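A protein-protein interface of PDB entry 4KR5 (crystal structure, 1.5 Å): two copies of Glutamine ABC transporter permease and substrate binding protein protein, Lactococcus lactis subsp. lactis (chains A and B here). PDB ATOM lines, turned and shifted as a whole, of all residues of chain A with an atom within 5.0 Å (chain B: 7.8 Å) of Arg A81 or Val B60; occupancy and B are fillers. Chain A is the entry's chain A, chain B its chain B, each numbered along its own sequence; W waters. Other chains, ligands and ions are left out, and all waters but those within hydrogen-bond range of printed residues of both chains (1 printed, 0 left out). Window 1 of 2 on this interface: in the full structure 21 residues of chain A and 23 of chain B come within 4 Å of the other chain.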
ATOM      1  N   PHE A  56      12.127  -9.018 -27.972  1.00  0.00           N
ATOM      2  CA  PHE A  56      12.224  -7.713 -27.293  1.00  0.00           C
ATOM      3  C   PHE A  56      11.625  -6.543 -28.083  1.00  0.00           C
ATOM      4  O   PHE A  56      10.770  -5.816 -27.554  1.00  0.00           O
ATOM      5  CB  PHE A  56      13.682  -7.430 -26.923  1.00  0.00           C
ATOM      6  CG  PHE A  56      13.857  -6.272 -25.978  1.00  0.00           C
ATOM      7  CD1 PHE A  56      13.816  -4.962 -26.449  1.00  0.00           C
ATOM      8  CD2 PHE A  56      14.002  -6.490 -24.612  1.00  0.00           C
ATOM      9  CE1 PHE A  56      13.970  -3.886 -25.575  1.00  0.00           C
ATOM     10  CE2 PHE A  56      14.153  -5.420 -23.736  1.00  0.00           C
ATOM     11  CZ  PHE A  56      14.114  -4.112 -24.223  1.00  0.00           C
ATOM     12  N   MET A  75      14.652  -6.286 -18.859  1.00  0.00           N
ATOM     13  CA  MET A  75      14.596  -4.946 -19.444  1.00  0.00           C
ATOM     14  C   MET A  75      15.322  -3.939 -18.572  1.00  0.00           C
ATOM     15  O   MET A  75      14.872  -3.629 -17.472  1.00  0.00           O
ATOM     16  CB  MET A  75      13.161  -4.484 -19.620  1.00  0.00           C
ATOM     17  CG  MET A  75      13.005  -3.308 -20.535  1.00  0.00           C
ATOM     18  SD  MET A  75      11.258  -2.878 -20.710  1.00  0.00           S
ATOM     19  CE  MET A  75      11.150  -2.257 -22.380  1.00  0.00           C
ATOM     20  N   SER A  76      16.447  -3.438 -19.066  1.00  0.00           N
ATOM     21  CA  SER A  76      17.186  -2.398 -18.362  1.00  0.00           C
ATOM     22  C   SER A  76      16.375  -1.116 -18.251  1.00  0.00           C
ATOM     23  O   SER A  76      15.879  -0.588 -19.246  1.00  0.00           O
ATOM     24  CB  SER A  76      18.514  -2.107 -19.063  1.00  0.00           C
ATOM     25  OG  SER A  76      19.337  -3.273 -19.127  1.00  0.00           O
ATOM     26  N   THR A  78      16.034   2.629 -18.168  1.00  0.00           N
ATOM     27  CA  THR A  78      16.828   3.741 -18.645  1.00  0.00           C
ATOM     28  C   THR A  78      15.942   4.944 -18.759  1.00  0.00           C
ATOM     29  O   THR A  78      14.720   4.815 -18.810  1.00  0.00           O
ATOM     30  CB  THR A  78      17.366   3.491 -20.065  1.00  0.00           C
ATOM     31  OG1 THR A  78      16.270   3.320 -20.976  1.00  0.00           O
ATOM     32  CG2 THR A  78      18.235   2.241 -20.080  1.00  0.00           C
ATOM     33  N   ASP A  79      16.564   6.113 -18.885  1.00  0.00           N
ATOM     34  CA  ASP A  79      15.806   7.328 -19.043  1.00  0.00           C
ATOM     35  C   ASP A  79      15.004   7.314 -20.336  1.00  0.00           C
ATOM     36  O   ASP A  79      13.856   7.762 -20.361  1.00  0.00           O
ATOM     37  CB  ASP A  79      16.715   8.547 -19.032  1.00  0.00           C
ATOM     38  CG  ASP A  79      15.930   9.815 -18.969  1.00  0.00           C
ATOM     39  OD1 ASP A  79      15.271  10.028 -17.918  1.00  0.00           O
ATOM     40  OD2 ASP A  79      15.935  10.576 -19.970  1.00  0.00           O
ATOM     41  N   ALA A  80      15.592   6.776 -21.398  1.00  0.00           N
ATOM     42  CA  ALA A  80      14.899   6.714 -22.681  1.00  0.00           C
ATOM     43  C   ALA A  80      13.646   5.855 -22.568  1.00  0.00           C
ATOM     44  O   ALA A  80      12.610   6.175 -23.147  1.00  0.00           O
ATOM     45  CB  ALA A  80      15.824   6.183 -23.785  1.00  0.00           C
ATOM     46  N   ARG A  81      13.721   4.754 -21.835  1.00  0.00           N
ATOM     47  CA  ARG A  81      12.548   3.909 -21.652  1.00  0.00           C
ATOM     48  C   ARG A  81      11.516   4.567 -20.768  1.00  0.00           C
ATOM     49  O   ARG A  81      10.321   4.385 -20.981  1.00  0.00           O
ATOM     50  CB  ARG A  81      12.935   2.521 -21.121  1.00  0.00           C
ATOM     51  CG  ARG A  81      13.627   1.698 -22.201  1.00  0.00           C
ATOM     52  CD  ARG A  81      13.981   0.263 -21.825  1.00  0.00           C
ATOM     53  NE  ARG A  81      14.665  -0.276 -22.993  1.00  0.00           N
ATOM     54  CZ  ARG A  81      15.976  -0.517 -23.096  1.00  0.00           C
ATOM     55  NH1 ARG A  81      16.782  -0.425 -22.055  1.00  0.00           N
ATOM     56  NH2 ARG A  81      16.487  -0.871 -24.270  1.00  0.00           N
ATOM     57  N   LYS A  82      11.964   5.353 -19.793  1.00  0.00           N
ATOM     58  CA  LYS A  82      11.020   6.068 -18.950  1.00  0.00           C
ATOM     59  C   LYS A  82      10.217   7.128 -19.711  1.00  0.00           C
ATOM     60  O   LYS A  82       9.217   7.638 -19.193  1.00  0.00           O
ATOM     61  CB  LYS A  82      11.730   6.698 -17.758  1.00  0.00           C
ATOM     62  CG  LYS A  82      12.148   5.667 -16.730  1.00  0.00           C
ATOM     63  CD  LYS A  82      12.849   6.298 -15.568  1.00  0.00           C
ATOM     64  CE  LYS A  82      13.034   5.310 -14.464  1.00  0.00           C
ATOM     65  NZ  LYS A  82      13.573   5.971 -13.275  1.00  0.00           N
ATOM     66  N   GLN A  83      10.631   7.437 -20.939  1.00  0.00           N
ATOM     67  CA  GLN A  83       9.868   8.353 -21.783  1.00  0.00           C
ATOM     68  C   GLN A  83       8.520   7.764 -22.159  1.00  0.00           C
ATOM     69  O   GLN A  83       7.559   8.494 -22.333  1.00  0.00           O
ATOM     70  CB  GLN A  83      10.624   8.693 -23.075  1.00  0.00           C
ATOM     71  CG  GLN A  83      12.001   9.272 -22.848  1.00  0.00           C
ATOM     72  CD  GLN A  83      11.959  10.537 -22.044  1.00  0.00           C
ATOM     73  OE1 GLN A  83      11.274  11.486 -22.420  1.00  0.00           O
ATOM     74  NE2 GLN A  83      12.662  10.559 -20.923  1.00  0.00           N
ATOM     75  N   VAL A  84       8.452   6.447 -22.289  1.00  0.00           N
ATOM     76  CA  VAL A  84       7.286   5.792 -22.858  1.00  0.00           C
ATOM     77  C   VAL A  84       6.733   4.626 -22.029  1.00  0.00           C
ATOM     78  O   VAL A  84       5.689   4.067 -22.383  1.00  0.00           O
ATOM     79  CB  VAL A  84       7.579   5.290 -24.291  1.00  0.00           C
ATOM     80  CG1 VAL A  84       7.798   6.485 -25.230  1.00  0.00           C
ATOM     81  CG2 VAL A  84       8.753   4.321 -24.317  1.00  0.00           C
ATOM     82  N   PHE A  85       7.431   4.264 -20.955  1.00  0.00           N
ATOM     83  CA  PHE A  85       6.976   3.208 -20.044  1.00  0.00           C
ATOM     84  C   PHE A  85       6.947   3.676 -18.598  1.00  0.00           C
ATOM     85  O   PHE A  85       7.770   4.499 -18.186  1.00  0.00           O
ATOM     86  CB  PHE A  85       7.941   1.998 -20.039  1.00  0.00           C
ATOM     87  CG  PHE A  85       7.977   1.193 -21.334  1.00  0.00           C
ATOM     88  CD1 PHE A  85       6.975   0.280 -21.620  1.00  0.00           C
ATOM     89  CD2 PHE A  85       9.035   1.327 -22.240  1.00  0.00           C
ATOM     90  CE1 PHE A  85       7.011  -0.482 -22.801  1.00  0.00           C
ATOM     91  CE2 PHE A  85       9.069   0.583 -23.422  1.00  0.00           C
ATOM     92  CZ  PHE A  85       8.066  -0.328 -23.699  1.00  0.00           C
ATOM     93  N   TYR A  87       7.535   1.846 -14.800  1.00  0.00           N
ATOM     94  CA  TYR A  87       8.197   0.674 -14.227  1.00  0.00           C
ATOM     95  C   TYR A  87       7.726   0.387 -12.833  1.00  0.00           C
ATOM     96  O   TYR A  87       7.427   1.306 -12.056  1.00  0.00           O
ATOM     97  CB  TYR A  87       9.717   0.889 -14.198  1.00  0.00           C
ATOM     98  CG  TYR A  87      10.310   0.681 -15.572  1.00  0.00           C
ATOM     99  CD1 TYR A  87      10.573  -0.614 -16.029  1.00  0.00           C
ATOM    100  CD2 TYR A  87      10.570   1.757 -16.419  1.00  0.00           C
ATOM    101  CE1 TYR A  87      11.086  -0.837 -17.289  1.00  0.00           C
ATOM    102  CE2 TYR A  87      11.093   1.537 -17.689  1.00  0.00           C
ATOM    103  CZ  TYR A  87      11.337   0.244 -18.115  1.00  0.00           C
ATOM    104  OH  TYR A  87      11.835   0.037 -19.379  1.00  0.00           O
ATOM    105  N   ALA B  13      25.910  -0.550 -33.937  1.00  0.00           N
ATOM    106  CA  ALA B  13      25.379  -1.627 -33.097  1.00  0.00           C
ATOM    107  C   ALA B  13      24.219  -2.323 -33.794  1.00  0.00           C
ATOM    108  O   ALA B  13      23.445  -1.700 -34.514  1.00  0.00           O
ATOM    109  CB  ALA B  13      24.948  -1.103 -31.747  1.00  0.00           C
ATOM    110  N   SER B  14      24.114  -3.625 -33.576  1.00  0.00           N
ATOM    111  CA  SER B  14      23.093  -4.423 -34.229  1.00  0.00           C
ATOM    112  C   SER B  14      22.722  -5.647 -33.387  1.00  0.00           C
ATOM    113  O   SER B  14      23.385  -6.001 -32.422  1.00  0.00           O
ATOM    114  CB  SER B  14      23.599  -4.878 -35.597  1.00  0.00           C
ATOM    115  OG  SER B  14      22.593  -5.518 -36.364  1.00  0.00           O
ATOM    116  N   ASP B  15      21.658  -6.315 -33.805  1.00  0.00           N
ATOM    117  CA  ASP B  15      21.245  -7.566 -33.195  1.00  0.00           C
ATOM    118  C   ASP B  15      22.300  -8.628 -33.502  1.00  0.00           C
ATOM    119  O   ASP B  15      23.063  -8.487 -34.444  1.00  0.00           O
ATOM    120  CB  ASP B  15      19.910  -7.979 -33.820  1.00  0.00           C
ATOM    121  CG  ASP B  15      19.075  -8.855 -32.928  1.00  0.00           C
ATOM    122  OD1 ASP B  15      19.626  -9.663 -32.167  1.00  0.00           O
ATOM    123  OD2 ASP B  15      17.836  -8.750 -33.023  1.00  0.00           O
ATOM    124  N   ILE B  54      25.398  -7.115 -30.888  1.00  0.00           N
ATOM    125  CA  ILE B  54      25.245  -7.312 -29.442  1.00  0.00           C
ATOM    126  C   ILE B  54      23.827  -7.641 -28.966  1.00  0.00           C
ATOM    127  O   ILE B  54      23.649  -8.063 -27.814  1.00  0.00           O
ATOM    128  CB  ILE B  54      25.795  -6.105 -28.675  1.00  0.00           C
ATOM    129  CG1 ILE B  54      25.149  -4.812 -29.171  1.00  0.00           C
ATOM    130  CG2 ILE B  54      27.309  -6.035 -28.850  1.00  0.00           C
ATOM    131  CD1 ILE B  54      25.551  -3.561 -28.387  1.00  0.00           C
ATOM    132  N   GLY B  55      22.837  -7.440 -29.843  1.00  0.00           N
ATOM    133  CA  GLY B  55      21.436  -7.696 -29.533  1.00  0.00           C
ATOM    134  C   GLY B  55      20.637  -6.418 -29.608  1.00  0.00           C
ATOM    135  O   GLY B  55      21.209  -5.338 -29.482  1.00  0.00           O
ATOM    136  N   PHE B  56      19.320  -6.529 -29.812  1.00  0.00           N
ATOM    137  CA  PHE B  56      18.505  -5.355 -30.044  1.00  0.00           C
ATOM    138  C   PHE B  56      18.521  -4.395 -28.843  1.00  0.00           C
ATOM    139  O   PHE B  56      18.831  -3.216 -28.988  1.00  0.00           O
ATOM    140  CB  PHE B  56      17.063  -5.740 -30.374  1.00  0.00           C
ATOM    141  CG  PHE B  56      16.197  -4.552 -30.615  1.00  0.00           C
ATOM    142  CD1 PHE B  56      16.092  -4.013 -31.883  1.00  0.00           C
ATOM    143  CD2 PHE B  56      15.522  -3.929 -29.570  1.00  0.00           C
ATOM    144  CE1 PHE B  56      15.321  -2.889 -32.110  1.00  0.00           C
ATOM    145  CE2 PHE B  56      14.730  -2.797 -29.813  1.00  0.00           C
ATOM    146  CZ  PHE B  56      14.637  -2.292 -31.080  1.00  0.00           C
ATOM    147  N   GLN B  57      18.183  -4.898 -27.661  1.00  0.00           N
ATOM    148  CA  GLN B  57      18.139  -4.036 -26.485  1.00  0.00           C
ATOM    149  C   GLN B  57      19.500  -3.376 -26.243  1.00  0.00           C
ATOM    150  O   GLN B  57      19.581  -2.180 -25.969  1.00  0.00           O
ATOM    151  CB  GLN B  57      17.729  -4.804 -25.222  1.00  0.00           C
ATOM    152  CG  GLN B  57      17.767  -3.887 -23.983  1.00  0.00           C
ATOM    153  CD  GLN B  57      17.260  -4.503 -22.679  1.00  0.00           C
ATOM    154  OE1 GLN B  57      16.902  -3.769 -21.767  1.00  0.00           O
ATOM    155  NE2 GLN B  57      17.244  -5.829 -22.585  1.00  0.00           N
ATOM    156  N   ALA B  58      20.550  -4.182 -26.303  1.00  0.00           N
ATOM    157  CA  ALA B  58      21.907  -3.711 -26.066  1.00  0.00           C
ATOM    158  C   ALA B  58      22.318  -2.637 -27.092  1.00  0.00           C
ATOM    159  O   ALA B  58      23.009  -1.661 -26.757  1.00  0.00           O
ATOM    160  CB  ALA B  58      22.868  -4.884 -26.107  1.00  0.00           C
ATOM    161  N   ALA B  59      21.897  -2.829 -28.333  1.00  0.00           N
ATOM    162  CA  ALA B  59      22.206  -1.895 -29.409  1.00  0.00           C
ATOM    163  C   ALA B  59      21.509  -0.543 -29.178  1.00  0.00           C
ATOM    164  O   ALA B  59      22.113   0.521 -29.357  1.00  0.00           O
ATOM    165  CB  ALA B  59      21.796  -2.503 -30.751  1.00  0.00           C
ATOM    166  N   VAL B  60      20.238  -0.581 -28.787  1.00  0.00           N
ATOM    167  CA  VAL B  60      19.527   0.642 -28.434  1.00  0.00           C
ATOM    168  C   VAL B  60      20.297   1.393 -27.346  1.00  0.00           C
ATOM    169  O   VAL B  60      20.521   2.612 -27.436  1.00  0.00           O
ATOM    170  CB  VAL B  60      18.090   0.343 -27.937  1.00  0.00           C
ATOM    171  CG1 VAL B  60      17.471   1.570 -27.250  1.00  0.00           C
ATOM    172  CG2 VAL B  60      17.194  -0.126 -29.067  1.00  0.00           C
ATOM    173  N   ASP B  61      20.675   0.679 -26.295  1.00  0.00           N
ATOM    174  CA  ASP B  61      21.283   1.349 -25.152  1.00  0.00           C
ATOM    175  C   ASP B  61      22.701   1.833 -25.461  1.00  0.00           C
ATOM    176  O   ASP B  61      23.174   2.825 -24.879  1.00  0.00           O
ATOM    177  CB  ASP B  61      21.257   0.444 -23.927  1.00  0.00           C
ATOM    178  CG  ASP B  61      19.844   0.161 -23.453  1.00  0.00           C
ATOM    179  OD1 ASP B  61      18.896   0.722 -24.050  1.00  0.00           O
ATOM    180  OD2 ASP B  61      19.694  -0.592 -22.471  1.00  0.00           O
ATOM    181  N   SER B  62      23.384   1.145 -26.371  1.00  0.00           N
ATOM    182  CA  SER B  62      24.722   1.562 -26.775  1.00  0.00           C
ATOM    183  C   SER B  62      24.663   2.862 -27.568  1.00  0.00           C
ATOM    184  O   SER B  62      25.468   3.773 -27.350  1.00  0.00           O
ATOM    185  CB  SER B  62      25.401   0.458 -27.594  1.00  0.00           C
ATOM    186  OG  SER B  62      26.709   0.863 -27.974  1.00  0.00           O
ATOM    187  N   VAL B  63      23.703   2.980 -28.482  1.00  0.00           N
ATOM    188  CA  VAL B  63      23.580   4.234 -29.228  1.00  0.00           C
ATOM    189  C   VAL B  63      23.176   5.365 -28.288  1.00  0.00           C
ATOM    190  O   VAL B  63      23.715   6.477 -28.353  1.00  0.00           O
ATOM    191  CB  VAL B  63      22.606   4.117 -30.407  1.00  0.00           C
ATOM    192  CG1 VAL B  63      22.364   5.493 -31.076  1.00  0.00           C
ATOM    193  CG2 VAL B  63      23.175   3.140 -31.429  1.00  0.00           C
ATOM    194  N   GLN B  64      22.239   5.087 -27.396  1.00  0.00           N
ATOM    195  CA  GLN B  64      21.759   6.152 -26.513  1.00  0.00           C
ATOM    196  C   GLN B  64      22.849   6.646 -25.549  1.00  0.00           C
ATOM    197  O   GLN B  64      22.803   7.790 -25.098  1.00  0.00           O
ATOM    198  CB  GLN B  64      20.529   5.704 -25.717  1.00  0.00           C
ATOM    199  CG  GLN B  64      19.280   5.530 -26.566  1.00  0.00           C
ATOM    200  CD  GLN B  64      18.782   6.845 -27.142  1.00  0.00           C
ATOM    201  OE1 GLN B  64      18.735   7.870 -26.450  1.00  0.00           O
ATOM    202  NE2 GLN B  64      18.425   6.824 -28.416  1.00  0.00           N
ATOM    203  N   SER B  65      23.795   5.776 -25.198  1.00  0.00           N
ATOM    204  CA  SER B  65      24.839   6.132 -24.242  1.00  0.00           C
ATOM    205  C   SER B  65      26.098   6.655 -24.922  1.00  0.00           C
ATOM    206  O   SER B  65      27.068   7.049 -24.249  1.00  0.00           O
ATOM    207  CB  SER B  65      25.184   4.933 -23.364  1.00  0.00           C
ATOM    208  OG  SER B  65      25.769   3.896 -24.129  1.00  0.00           O
ATOM    209  N   GLY B  66      26.084   6.651 -26.248  1.00  0.00           N
ATOM    210  CA  GLY B  66      27.201   7.160 -27.024  1.00  0.00           C
ATOM    211  C   GLY B  66      28.294   6.139 -27.299  1.00  0.00           C
ATOM    212  O   GLY B  66      29.349   6.485 -27.849  1.00  0.00           O
ATOM    213  N   ALA B  68      27.947   3.621 -29.308  1.00  0.00           N
ATOM    214  CA  ALA B  68      27.857   3.336 -30.736  1.00  0.00           C
ATOM    215  C   ALA B  68      27.311   4.565 -31.427  1.00  0.00           C
ATOM    216  O   ALA B  68      26.595   5.343 -30.816  1.00  0.00           O
ATOM    217  CB  ALA B  68      26.943   2.150 -30.975  1.00  0.00           C
ATOM    218  N   GLY B  70      25.620   4.502 -34.587  1.00  0.00           N
ATOM    219  CA  GLY B  70      24.388   4.209 -35.292  1.00  0.00           C
ATOM    220  C   GLY B  70      23.892   2.807 -35.003  1.00  0.00           C
ATOM    221  O   GLY B  70      24.617   1.960 -34.473  1.00  0.00           O
ATOM    222  N   MET B  71      22.641   2.569 -35.377  1.00  0.00           N
ATOM    223  CA  MET B  71      22.028   1.260 -35.207  1.00  0.00           C
ATOM    224  C   MET B  71      21.360   0.822 -36.505  1.00  0.00           C
ATOM    225  O   MET B  71      20.554   1.559 -37.090  1.00  0.00           O
ATOM    226  CB  MET B  71      20.991   1.307 -34.076  1.00  0.00           C
ATOM    227  CG  MET B  71      20.223   0.047 -33.885  1.00  0.00           C
ATOM    228  SD  MET B  71      19.429   0.104 -32.258  1.00  0.00           S
ATOM    229  CE  MET B  71      18.507  -1.422 -32.370  1.00  0.00           C
ATOM    230  N   SER B  73      19.527  -2.660 -37.559  1.00  0.00           N
ATOM    231  CA  SER B  73      19.128  -3.823 -36.766  1.00  0.00           C
ATOM    232  C   SER B  73      17.678  -4.217 -37.026  1.00  0.00           C
ATOM    233  O   SER B  73      16.949  -4.578 -36.091  1.00  0.00           O
ATOM    234  CB  SER B  73      19.336  -3.506 -35.269  1.00  0.00           C
ATOM    235  OG  SER B  73      19.259  -4.651 -34.445  1.00  0.00           O
ATOM    236  N   MET B  75      15.213  -2.440 -37.588  1.00  0.00           N
ATOM    237  CA  MET B  75      14.512  -1.604 -36.611  1.00  0.00           C
ATOM    238  C   MET B  75      13.275  -0.929 -37.177  1.00  0.00           C
ATOM    239  O   MET B  75      13.365  -0.095 -38.082  1.00  0.00           O
ATOM    240  CB  MET B  75      15.465  -0.547 -36.049  1.00  0.00           C
ATOM    241  CG  MET B  75      14.919   0.221 -34.873  1.00  0.00           C
ATOM    242  SD  MET B  75      16.155   1.378 -34.293  1.00  0.00           S
ATOM    243  CE  MET B  75      15.990   1.183 -32.518  1.00  0.00           C
ATOM    244  N   ARG B  81      10.094   5.529 -30.975  1.00  0.00           N
ATOM    245  CA  ARG B  81      11.527   5.534 -31.268  1.00  0.00           C
ATOM    246  C   ARG B  81      12.019   6.889 -31.732  1.00  0.00           C
ATOM    247  O   ARG B  81      13.143   7.277 -31.427  1.00  0.00           O
ATOM    248  CB  ARG B  81      11.890   4.453 -32.297  1.00  0.00           C
ATOM    249  CG  ARG B  81      12.020   3.123 -31.604  1.00  0.00           C
ATOM    250  CD  ARG B  81      12.275   1.917 -32.505  1.00  0.00           C
ATOM    251  NE  ARG B  81      12.081   0.759 -31.641  1.00  0.00           N
ATOM    252  CZ  ARG B  81      11.130  -0.163 -31.792  1.00  0.00           C
ATOM    253  NH1 ARG B  81      10.371  -0.205 -32.876  1.00  0.00           N
ATOM    254  NH2 ARG B  81      10.990  -1.099 -30.869  1.00  0.00           N
ATOM    255  N   VAL B  84      13.620   9.475 -29.388  1.00  0.00           N
ATOM    256  CA  VAL B  84      15.010   9.380 -28.932  1.00  0.00           C
ATOM    257  C   VAL B  84      16.038   9.078 -30.030  1.00  0.00           C
ATOM    258  O   VAL B  84      17.231   9.150 -29.770  1.00  0.00           O
ATOM    259  CB  VAL B  84      15.174   8.366 -27.750  1.00  0.00           C
ATOM    260  CG1 VAL B  84      14.382   8.832 -26.520  1.00  0.00           C
ATOM    261  CG2 VAL B  84      14.764   6.966 -28.160  1.00  0.00           C
ATOM    262  N   PHE B  85      15.571   8.764 -31.239  1.00  0.00           N
ATOM    263  CA  PHE B  85      16.439   8.535 -32.410  1.00  0.00           C
ATOM    264  C   PHE B  85      16.053   9.455 -33.576  1.00  0.00           C
ATOM    265  O   PHE B  85      14.887   9.839 -33.710  1.00  0.00           O
ATOM    266  CB  PHE B  85      16.281   7.086 -32.907  1.00  0.00           C
ATOM    267  CG  PHE B  85      16.837   6.035 -31.971  1.00  0.00           C
ATOM    268  CD1 PHE B  85      18.207   5.772 -31.931  1.00  0.00           C
ATOM    269  CD2 PHE B  85      15.984   5.275 -31.170  1.00  0.00           C
ATOM    270  CE1 PHE B  85      18.726   4.792 -31.094  1.00  0.00           C
ATOM    271  CE2 PHE B  85      16.487   4.285 -30.333  1.00  0.00           C
ATOM    272  CZ  PHE B  85      17.872   4.036 -30.295  1.00  0.00           C
ATOM    273  N   TYR B  87      16.210   9.106 -37.789  1.00  0.00           N
ATOM    274  CA  TYR B  87      16.273   8.030 -38.781  1.00  0.00           C
ATOM    275  C   TYR B  87      16.697   8.517 -40.148  1.00  0.00           C
ATOM    276  O   TYR B  87      16.366   9.638 -40.552  1.00  0.00           O
ATOM    277  CB  TYR B  87      14.899   7.367 -38.904  1.00  0.00           C
ATOM    278  CG  TYR B  87      14.633   6.429 -37.774  1.00  0.00           C
ATOM    279  CD1 TYR B  87      15.161   5.154 -37.790  1.00  0.00           C
ATOM    280  CD2 TYR B  87      13.870   6.817 -36.680  1.00  0.00           C
ATOM    281  CE1 TYR B  87      14.956   4.289 -36.741  1.00  0.00           C
ATOM    282  CE2 TYR B  87      13.646   5.955 -35.633  1.00  0.00           C
ATOM    283  CZ  TYR B  87      14.185   4.681 -35.676  1.00  0.00           C
ATOM    284  OH  TYR B  87      13.985   3.788 -34.634  1.00  0.00           O
ATOM    285  N   LYS B 196      21.423   8.470 -32.441  1.00  0.00           N
ATOM    286  CA  LYS B 196      20.815   9.132 -31.289  1.00  0.00           C
ATOM    287  C   LYS B 196      20.275  10.471 -31.768  1.00  0.00           C
ATOM    288  O   LYS B 196      20.906  11.152 -32.577  1.00  0.00           O
ATOM    289  CB  LYS B 196      21.846   9.338 -30.181  1.00  0.00           C
ATOM    290  CG  LYS B 196      21.248   9.887 -28.861  1.00  0.00           C
ATOM    291  CD  LYS B 196      22.318  10.032 -27.802  1.00  0.00           C
ATOM    292  CE  LYS B 196      21.756  10.606 -26.511  1.00  0.00           C
ATOM    293  NZ  LYS B 196      22.794  10.662 -25.456  1.00  0.00           N
HETATM  294  O   HOH W   1      16.901   2.707 -23.655  1.00  0.00           O
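Among the printed residues, merely in contact across the chains: Phe A56 with Gln B57 (3.3 Å), Met A75 with Gln B57 (3.5 Å), Phe A56 with Phe B56 (3.7 Å), Ser A76 with Asp B61 (3.9 Å), Arg A81 with Val B60 (3.98 Å) and Thr A78 with Asp B61 (3.98 Å).
Printed residues of chain B that touch a printed residue of chain A: Phe B56, Gln B57, Val B60 and Asp B61. Hydrophobic or aromatic side chains of chain B within 4 Å of the printed part of chain A: Phe B56 and Val B60. Of the 12 printed residues of chain A, 5 touch a printed residue of chain B. Hydrophobic or aromatic side chains of chain A within 4 Å of the printed part of chain B: Phe A56. Among the printed residues, 9 pairs touch across the chains.
OH of Tyr A87 is in hydrogen-bond range of SD of Met A75 (3.3 Å). O of Ser A76 lies within hydrogen-bond range of NH1 of Arg A81, 3.0 Å away. OG1 of Thr A78 sits at hydrogen-bond distance from N of Arg A81, 3.0 Å away. The backbone NH (N) of Val B60 is in hydrogen-bond range of the side-chain sulfur (SD) of Met B71 (3.6 Å). O of Asp B61 sits at hydrogen-bond distance from OG of Ser B65 (2.9 Å).
Water W1 lies within hydrogen-bond range of the side-chain hydroxyl (OG1) of Thr A78 (2.8 Å) and the side-chain carboxylate (OD1) of Asp B61 (2.8 Å).
The backbone NH (N) of Ser A76 is in hydrogen-bond range of the side-chain amide oxygen (OE1) of Gln B57. NH1 of Arg A81 lies within hydrogen-bond range of OE1 of Gln B57 (3.4 Å). The guanidinium group (NH2) of Arg A81 is in salt-bridge range of the side-chain carboxylate (OD1) of Asp B61, at 2.9 Å.
Phe B56 touches its own counterpart, Phe A56.
Arg A81 touches just these residues of chain B: Gln B57 (3.3 Å), Val B60 (3.98 Å) and Asp B61 (2.9 Å). Val B60 touches one residue of chain A. No residue of chain B comes within 4 Å of Ala A80. Of the printed residues of chain A, Asp B61 touches Ser A76, Thr A78 and Arg A81. Of the printed residues of chain B, Met A75 touches Gln B57 (3.5 Å). Printed residues of chain B within 4 Å of Thr A78: Asp B61 (3.98 Å). Tyr A87 touches none of the printed residues of chain B. The nearest residue of chain B that does not touch Arg A81 is Ala B58 (5.6 Å). The nearest printed residue of chain B that does not touch Ser A76 is Ala B58 (7.3 Å).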
